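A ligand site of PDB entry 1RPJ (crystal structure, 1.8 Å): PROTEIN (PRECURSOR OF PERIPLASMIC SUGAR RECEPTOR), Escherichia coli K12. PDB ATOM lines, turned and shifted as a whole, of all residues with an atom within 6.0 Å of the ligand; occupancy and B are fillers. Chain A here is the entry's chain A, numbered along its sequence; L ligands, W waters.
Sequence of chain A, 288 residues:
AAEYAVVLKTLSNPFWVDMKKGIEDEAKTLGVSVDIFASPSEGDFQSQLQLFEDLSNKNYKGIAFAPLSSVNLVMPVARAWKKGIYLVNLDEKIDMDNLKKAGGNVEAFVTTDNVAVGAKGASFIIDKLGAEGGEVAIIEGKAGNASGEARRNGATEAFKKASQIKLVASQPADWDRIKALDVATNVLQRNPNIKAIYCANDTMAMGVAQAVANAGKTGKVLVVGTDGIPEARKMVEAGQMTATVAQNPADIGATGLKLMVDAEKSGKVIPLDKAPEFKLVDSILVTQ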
ATOM      1  N   LYS A   9       8.656 -19.108   2.825  1.00  0.00           N
ATOM      2  CA  LYS A   9       8.799 -20.053   3.926  1.00  0.00           C
ATOM      3  C   LYS A   9       9.580 -21.281   3.546  1.00  0.00           C
ATOM      4  O   LYS A   9      10.638 -21.514   4.147  1.00  0.00           O
ATOM      5  CB  LYS A   9       7.402 -20.418   4.491  1.00  0.00           C
ATOM      6  CG  LYS A   9       6.733 -19.222   5.155  1.00  0.00           C
ATOM      7  CD  LYS A   9       5.601 -19.822   6.038  1.00  0.00           C
ATOM      8  CE  LYS A   9       4.696 -18.707   6.577  1.00  0.00           C
ATOM      9  NZ  LYS A   9       3.500 -19.309   7.259  1.00  0.00           N
ATOM     10  N   THR A  10       9.055 -22.171   2.700  1.00  0.00           N
ATOM     11  CA  THR A  10       9.767 -23.393   2.351  1.00  0.00           C
ATOM     12  C   THR A  10       9.245 -23.877   0.995  1.00  0.00           C
ATOM     13  O   THR A  10       8.045 -23.925   0.720  1.00  0.00           O
ATOM     14  CB  THR A  10       9.607 -24.504   3.409  1.00  0.00           C
ATOM     15  OG1 THR A  10       9.981 -25.804   2.896  1.00  0.00           O
ATOM     16  CG2 THR A  10       8.151 -24.539   3.831  1.00  0.00           C
ATOM     17  N   ASN A  13       6.567 -27.012   0.170  1.00  0.00           N
ATOM     18  CA  ASN A  13       5.124 -26.775   0.103  1.00  0.00           C
ATOM     19  C   ASN A  13       4.823 -26.077  -1.209  1.00  0.00           C
ATOM     20  O   ASN A  13       5.287 -24.978  -1.495  1.00  0.00           O
ATOM     21  CB  ASN A  13       4.734 -25.945   1.329  1.00  0.00           C
ATOM     22  CG  ASN A  13       3.296 -25.480   1.442  1.00  0.00           C
ATOM     23  OD1 ASN A  13       2.538 -25.656   0.500  1.00  0.00           O
ATOM     24  ND2 ASN A  13       2.956 -24.859   2.587  1.00  0.00           N
ATOM     25  N   PHE A  15       2.427 -24.235  -2.216  1.00  0.00           N
ATOM     26  CA  PHE A  15       1.985 -22.877  -2.067  1.00  0.00           C
ATOM     27  C   PHE A  15       3.171 -21.905  -2.279  1.00  0.00           C
ATOM     28  O   PHE A  15       3.010 -20.885  -2.928  1.00  0.00           O
ATOM     29  CB  PHE A  15       1.432 -22.690  -0.634  1.00  0.00           C
ATOM     30  CG  PHE A  15       1.010 -21.290  -0.325  1.00  0.00           C
ATOM     31  CD1 PHE A  15      -0.280 -20.863  -0.653  1.00  0.00           C
ATOM     32  CD2 PHE A  15       1.869 -20.409   0.309  1.00  0.00           C
ATOM     33  CE1 PHE A  15      -0.706 -19.603  -0.356  1.00  0.00           C
ATOM     34  CE2 PHE A  15       1.420 -19.129   0.585  1.00  0.00           C
ATOM     35  CZ  PHE A  15       0.129 -18.702   0.299  1.00  0.00           C
ATOM     36  N   TRP A  16       4.292 -22.187  -1.647  1.00  0.00           N
ATOM     37  CA  TRP A  16       5.485 -21.345  -1.742  1.00  0.00           C
ATOM     38  C   TRP A  16       6.130 -21.514  -3.112  1.00  0.00           C
ATOM     39  O   TRP A  16       6.654 -20.542  -3.635  1.00  0.00           O
ATOM     40  CB  TRP A  16       6.489 -21.611  -0.596  1.00  0.00           C
ATOM     41  CG  TRP A  16       5.767 -21.287   0.702  1.00  0.00           C
ATOM     42  CD1 TRP A  16       5.274 -22.169   1.584  1.00  0.00           C
ATOM     43  CD2 TRP A  16       5.415 -19.991   1.187  1.00  0.00           C
ATOM     44  NE1 TRP A  16       4.626 -21.499   2.600  1.00  0.00           N
ATOM     45  CE2 TRP A  16       4.700 -20.171   2.379  1.00  0.00           C
ATOM     46  CE3 TRP A  16       5.613 -18.688   0.712  1.00  0.00           C
ATOM     47  CZ2 TRP A  16       4.206 -19.087   3.092  1.00  0.00           C
ATOM     48  CZ3 TRP A  16       5.125 -17.633   1.429  1.00  0.00           C
ATOM     49  CH2 TRP A  16       4.413 -17.827   2.619  1.00  0.00           C
ATOM     50  N   GLU A  42       9.545 -25.883   7.584  1.00  0.00           N
ATOM     51  CA  GLU A  42       8.719 -25.054   8.458  1.00  0.00           C
ATOM     52  C   GLU A  42       9.343 -24.821   9.827  1.00  0.00           C
ATOM     53  O   GLU A  42       9.101 -23.740  10.387  1.00  0.00           O
ATOM     54  CB  GLU A  42       7.329 -25.672   8.715  1.00  0.00           C
ATOM     55  CG  GLU A  42       6.309 -25.351   7.651  1.00  0.00           C
ATOM     56  CD  GLU A  42       5.872 -23.945   7.542  1.00  0.00           C
ATOM     57  OE1 GLU A  42       5.884 -23.131   8.494  1.00  0.00           O
ATOM     58  OE2 GLU A  42       5.535 -23.538   6.395  1.00  0.00           O
ATOM     59  N   ASP A  91       2.138 -12.590   2.828  1.00  0.00           N
ATOM     60  CA  ASP A  91       1.346 -13.689   3.345  1.00  0.00           C
ATOM     61  C   ASP A  91       1.129 -13.732   4.848  1.00  0.00           C
ATOM     62  O   ASP A  91      -0.025 -13.717   5.296  1.00  0.00           O
ATOM     63  CB  ASP A  91       1.913 -15.020   2.828  1.00  0.00           C
ATOM     64  CG  ASP A  91       1.173 -16.238   3.421  1.00  0.00           C
ATOM     65  OD1 ASP A  91       0.023 -16.512   3.071  1.00  0.00           O
ATOM     66  OD2 ASP A  91       1.770 -16.906   4.294  1.00  0.00           O
ATOM     67  N   GLU A  92       2.186 -13.921   5.605  1.00  0.00           N
ATOM     68  CA  GLU A  92       2.209 -14.227   7.020  1.00  0.00           C
ATOM     69  C   GLU A  92       2.592 -12.967   7.789  1.00  0.00           C
ATOM     70  O   GLU A  92       3.781 -12.635   7.763  1.00  0.00           O
ATOM     71  CB  GLU A  92       3.255 -15.331   7.260  1.00  0.00           C
ATOM     72  CG  GLU A  92       3.368 -15.794   8.717  1.00  0.00           C
ATOM     73  CD  GLU A  92       2.087 -16.509   9.170  1.00  0.00           C
ATOM     74  OE1 GLU A  92       1.971 -17.725   8.929  1.00  0.00           O
ATOM     75  OE2 GLU A  92       1.270 -15.831   9.791  1.00  0.00           O
ATOM     76  N   ASN A 114      -7.531 -13.894   5.619  1.00  0.00           N
ATOM     77  CA  ASN A 114      -7.529 -15.168   6.294  1.00  0.00           C
ATOM     78  C   ASN A 114      -8.707 -15.424   7.216  1.00  0.00           C
ATOM     79  O   ASN A 114      -9.071 -16.554   7.450  1.00  0.00           O
ATOM     80  CB  ASN A 114      -6.173 -15.334   6.986  1.00  0.00           C
ATOM     81  CG  ASN A 114      -5.199 -15.717   5.867  1.00  0.00           C
ATOM     82  OD1 ASN A 114      -5.493 -16.611   5.084  1.00  0.00           O
ATOM     83  ND2 ASN A 114      -4.072 -14.978   5.799  1.00  0.00           N
ATOM     84  N   ASN A 145       0.736 -17.649  14.768  1.00  0.00           N
ATOM     85  CA  ASN A 145       0.925 -17.171  13.401  1.00  0.00           C
ATOM     86  C   ASN A 145      -0.343 -16.452  12.968  1.00  0.00           C
ATOM     87  O   ASN A 145      -1.406 -17.053  12.987  1.00  0.00           O
ATOM     88  CB  ASN A 145       1.218 -18.291  12.403  1.00  0.00           C
ATOM     89  CG  ASN A 145       2.709 -18.570  12.405  1.00  0.00           C
ATOM     90  OD1 ASN A 145       3.342 -18.397  13.470  1.00  0.00           O
ATOM     91  ND2 ASN A 145       3.261 -19.002  11.292  1.00  0.00           N
ATOM     92  N   SER A 147      -1.597 -15.902  10.099  1.00  0.00           N
ATOM     93  CA  SER A 147      -2.398 -16.531   9.023  1.00  0.00           C
ATOM     94  C   SER A 147      -3.359 -17.574   9.605  1.00  0.00           C
ATOM     95  O   SER A 147      -4.562 -17.531   9.351  1.00  0.00           O
ATOM     96  CB  SER A 147      -1.455 -17.181   8.025  1.00  0.00           C
ATOM     97  OG  SER A 147      -0.648 -18.152   8.659  1.00  0.00           O
ATOM     98  N   GLY A 148      -2.763 -18.457  10.397  1.00  0.00           N
ATOM     99  CA  GLY A 148      -3.563 -19.544  10.999  1.00  0.00           C
ATOM    100  C   GLY A 148      -4.562 -18.963  12.013  1.00  0.00           C
ATOM    101  O   GLY A 148      -5.707 -19.464  12.133  1.00  0.00           O
ATOM    102  N   ARG A 151      -7.569 -17.617  10.235  1.00  0.00           N
ATOM    103  CA  ARG A 151      -8.416 -18.716   9.751  1.00  0.00           C
ATOM    104  C   ARG A 151      -9.169 -19.333  10.929  1.00  0.00           C
ATOM    105  O   ARG A 151     -10.357 -19.594  10.857  1.00  0.00           O
ATOM    106  CB  ARG A 151      -7.584 -19.788   9.041  1.00  0.00           C
ATOM    107  CG  ARG A 151      -6.964 -19.162   7.788  1.00  0.00           C
ATOM    108  CD  ARG A 151      -5.991 -20.174   7.150  1.00  0.00           C
ATOM    109  NE  ARG A 151      -5.256 -19.366   6.159  1.00  0.00           N
ATOM    110  CZ  ARG A 151      -4.035 -19.652   5.703  1.00  0.00           C
ATOM    111  NH1 ARG A 151      -3.439 -20.811   5.982  1.00  0.00           N
ATOM    112  NH2 ARG A 151      -3.490 -18.777   4.890  1.00  0.00           N
ATOM    113  N   TRP A 175       1.362 -26.521  10.835  1.00  0.00           N
ATOM    114  CA  TRP A 175       1.565 -26.664   9.401  1.00  0.00           C
ATOM    115  C   TRP A 175       2.286 -27.948   9.038  1.00  0.00           C
ATOM    116  O   TRP A 175       2.944 -28.058   7.977  1.00  0.00           O
ATOM    117  CB  TRP A 175       2.437 -25.495   8.894  1.00  0.00           C
ATOM    118  CG  TRP A 175       2.075 -24.107   9.305  1.00  0.00           C
ATOM    119  CD1 TRP A 175       2.880 -23.232   9.980  1.00  0.00           C
ATOM    120  CD2 TRP A 175       0.854 -23.411   9.105  1.00  0.00           C
ATOM    121  NE1 TRP A 175       2.244 -22.047  10.231  1.00  0.00           N
ATOM    122  CE2 TRP A 175       0.973 -22.130   9.684  1.00  0.00           C
ATOM    123  CE3 TRP A 175      -0.380 -23.776   8.531  1.00  0.00           C
ATOM    124  CZ2 TRP A 175      -0.039 -21.186   9.633  1.00  0.00           C
ATOM    125  CZ3 TRP A 175      -1.361 -22.839   8.483  1.00  0.00           C
ATOM    126  CH2 TRP A 175      -1.227 -21.554   9.056  1.00  0.00           C
ATOM    127  N   ALA A 200      -6.270 -25.482   8.851  1.00  0.00           N
ATOM    128  CA  ALA A 200      -5.758 -24.184   8.433  1.00  0.00           C
ATOM    129  C   ALA A 200      -4.851 -24.246   7.210  1.00  0.00           C
ATOM    130  O   ALA A 200      -4.617 -23.196   6.589  1.00  0.00           O
ATOM    131  CB  ALA A 200      -5.072 -23.468   9.602  1.00  0.00           C
ATOM    132  N   ASN A 201      -4.430 -25.411   6.757  1.00  0.00           N
ATOM    133  CA  ASN A 201      -3.758 -25.551   5.472  1.00  0.00           C
ATOM    134  C   ASN A 201      -3.820 -26.998   4.989  1.00  0.00           C
ATOM    135  O   ASN A 201      -4.189 -27.918   5.688  1.00  0.00           O
ATOM    136  CB  ASN A 201      -2.353 -24.993   5.360  1.00  0.00           C
ATOM    137  CG  ASN A 201      -1.240 -25.883   5.819  1.00  0.00           C
ATOM    138  OD1 ASN A 201      -1.425 -26.910   6.465  1.00  0.00           O
ATOM    139  ND2 ASN A 201      -0.017 -25.464   5.443  1.00  0.00           N
ATOM    140  N   ASP A 202      -3.452 -27.151   3.718  1.00  0.00           N
ATOM    141  CA  ASP A 202      -3.536 -28.422   3.012  1.00  0.00           C
ATOM    142  C   ASP A 202      -2.520 -29.425   3.510  1.00  0.00           C
ATOM    143  O   ASP A 202      -2.789 -30.640   3.575  1.00  0.00           O
ATOM    144  CB  ASP A 202      -3.394 -28.196   1.505  1.00  0.00           C
ATOM    145  CG  ASP A 202      -4.651 -27.603   0.888  1.00  0.00           C
ATOM    146  OD1 ASP A 202      -5.739 -27.603   1.511  1.00  0.00           O
ATOM    147  OD2 ASP A 202      -4.547 -27.134  -0.267  1.00  0.00           O
ATOM    148  N   THR A 203      -1.294 -28.940   3.786  1.00  0.00           N
ATOM    149  CA  THR A 203      -0.325 -29.885   4.341  1.00  0.00           C
ATOM    150  C   THR A 203      -0.949 -30.635   5.533  1.00  0.00           C
ATOM    151  O   THR A 203      -0.796 -31.854   5.602  1.00  0.00           O
ATOM    152  CB  THR A 203       0.898 -29.126   4.858  1.00  0.00           C
ATOM    153  OG1 THR A 203       1.372 -28.326   3.754  1.00  0.00           O
ATOM    154  CG2 THR A 203       1.945 -30.121   5.311  1.00  0.00           C
ATOM    155  N   THR A 226      -6.886 -25.726   3.246  1.00  0.00           N
ATOM    156  CA  THR A 226      -6.739 -24.336   2.751  1.00  0.00           C
ATOM    157  C   THR A 226      -5.428 -24.273   1.975  1.00  0.00           C
ATOM    158  O   THR A 226      -4.456 -24.876   2.453  1.00  0.00           O
ATOM    159  CB  THR A 226      -6.760 -23.355   3.913  1.00  0.00           C
ATOM    160  OG1 THR A 226      -8.098 -23.108   4.338  1.00  0.00           O
ATOM    161  CG2 THR A 226      -6.182 -21.970   3.517  1.00  0.00           C
ATOM    162  N   ASP A 227      -5.337 -23.595   0.877  1.00  0.00           N
ATOM    163  CA  ASP A 227      -4.233 -23.303  -0.020  1.00  0.00           C
ATOM    164  C   ASP A 227      -4.592 -23.684  -1.468  1.00  0.00           C
ATOM    165  O   ASP A 227      -4.330 -22.911  -2.398  1.00  0.00           O
ATOM    166  CB  ASP A 227      -2.842 -23.913   0.232  1.00  0.00           C
ATOM    167  CG  ASP A 227      -2.192 -23.433   1.548  1.00  0.00           C
ATOM    168  OD1 ASP A 227      -2.795 -22.460   2.069  1.00  0.00           O
ATOM    169  OD2 ASP A 227      -1.196 -24.061   1.952  1.00  0.00           O
ATOM    170  N   GLN A 247      -5.914 -20.611  -2.314  1.00  0.00           N
ATOM    171  CA  GLN A 247      -5.380 -19.249  -2.286  1.00  0.00           C
ATOM    172  C   GLN A 247      -4.701 -19.064  -3.672  1.00  0.00           C
ATOM    173  O   GLN A 247      -4.542 -20.042  -4.380  1.00  0.00           O
ATOM    174  CB  GLN A 247      -4.327 -19.029  -1.216  1.00  0.00           C
ATOM    175  CG  GLN A 247      -4.837 -19.224   0.220  1.00  0.00           C
ATOM    176  CD  GLN A 247      -3.793 -18.757   1.230  1.00  0.00           C
ATOM    177  OE1 GLN A 247      -3.592 -17.562   1.377  1.00  0.00           O
ATOM    178  NE2 GLN A 247      -3.113 -19.684   1.892  1.00  0.00           N
HETATM  179  C1  LIG L   1       0.473 -19.652   5.483  1.00  0.00           C
HETATM  180  C2  LIG L   1       0.163 -19.621   3.962  1.00  0.00           C
HETATM  181  C3  LIG L   1      -0.181 -21.029   3.479  1.00  0.00           C
HETATM  182  C4  LIG L   1       0.991 -21.966   3.791  1.00  0.00           C
HETATM  183  C5  LIG L   1       1.280 -21.880   5.294  1.00  0.00           C
HETATM  184  C6  LIG L   1       2.350 -22.797   5.800  1.00  0.00           C
HETATM  185  O1  LIG L   1       0.808 -18.373   5.967  1.00  0.00           O
HETATM  186  O2  LIG L   1      -0.925 -18.752   3.733  1.00  0.00           O
HETATM  187  O3  LIG L   1      -1.350 -21.488   4.230  1.00  0.00           O
HETATM  188  O4  LIG L   1       0.692 -23.327   3.483  1.00  0.00           O
HETATM  189  O5  LIG L   1       1.548 -20.543   5.694  1.00  0.00           O
HETATM  190  O6  LIG L   1       3.628 -22.512   5.185  1.00  0.00           O
HETATM  191  O   HOH W   1       4.901 -25.544   4.655  1.00  0.00           O
HETATM  192  O   HOH W   2      -2.493 -15.789   3.180  1.00  0.00           O
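OD2 of Asp 91 is in hydrogen-bond range of O1 of the ligand, 2.4 Å away.
O6 of the ligand sits at hydrogen-bond distance from OE2 of Glu 42, 2.5 Å away.
The side-chain carboxylate (OD2) of Asp 227 lies within hydrogen-bond range of an oxygen (O4) of the ligand, at 2.5 Å.
The side-chain amino group (NZ) of Lys 9 lies within hydrogen-bond range of an oxygen (O5) of the ligand (2.8 Å).
An oxygen (O3) of the ligand is in hydrogen-bond range of the guanidinium group of Arg 151 (2.8 Å).
The side-chain amide nitrogen of Asn 13 sits at hydrogen-bond distance from an oxygen (O4) of the ligand (2.9 Å).
The indole nitrogen (NE1) of Trp 16 is in hydrogen-bond range of an oxygen (O6) of the ligand (3.0 Å).
The side-chain amide nitrogen (ND2) of Asn 201 is in hydrogen-bond range of an oxygen (O4) of the ligand (3.0 Å).
The side-chain amide nitrogen (NE2) of Gln 247 lies within hydrogen-bond range of an oxygen (O2) of the ligand, at 3.0 Å.
An oxygen (O1) of the ligand lies within hydrogen-bond range of the side-chain hydroxyl of Ser 147, 3.1 Å away.
The side-chain carboxylate of Glu 92 sits at hydrogen-bond distance from an oxygen (O1) of the ligand.
The backbone carbonyl oxygen of Asp 227 lies within hydrogen-bond range of the backbone NH of Gln 247 (2.8 Å).
NZ of Lys 9 lies within salt-bridge range of OE1 of Glu 92, 2.8 Å away.
NE2 of Gln 247 lies close to NH2 of Arg 151 (3.2 Å).
The backbone carbonyl oxygen (O) of Ala 200 is in hydrogen-bond range of the guanidinium group (NH1) of Arg 151 (2.7 Å).
The guanidinium group (NH2) of Arg 151 is in hydrogen-bond range of the side-chain amide oxygen (OD1) of Asn 114 (3.0 Å).
The side-chain amide oxygen (OD1) of Asn 13 sits at hydrogen-bond distance from the backbone NH (N) of Phe 15 (3.1 Å).
OD1 of Asn 201 is in hydrogen-bond range of N of Thr 203 (3.4 Å).
The side-chain hydroxyl (OG) of Ser 147 is in hydrogen-bond range of the side-chain carboxylate (OE1) of Glu 92 (2.7 Å).
CZ of Phe 15 touches O2 of the ligand, 3.6 Å away.
Trp 175 touches the ligand (CD2 to C6, 3.7 Å).
Hydrophobic or aromatic side chains within 4 Å of the ligand: Phe 15, Trp 16 and Trp 175.
13 residues have an atom within 4 Å of the ligand: Lys 9, Asn 13, Phe 15, Trp 16, Glu 42, Asp 91, Glu 92, Ser 147, Arg 151, Trp 175, Asn 201, Asp 227 and Gln 247.
Water W1 lies within hydrogen-bond range of OE2 of Glu 42 (2.7 Å), ND2 of Asn 13 (2.9 Å) and O6 of the ligand (3.3 Å).
Water W2 lies within hydrogen-bond range of OD1 of Asp 91 (2.6 Å), OE1 of Gln 247 (2.8 Å), ND2 of Asn 114 (3.2 Å) and O2 of the ligand (3.4 Å).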
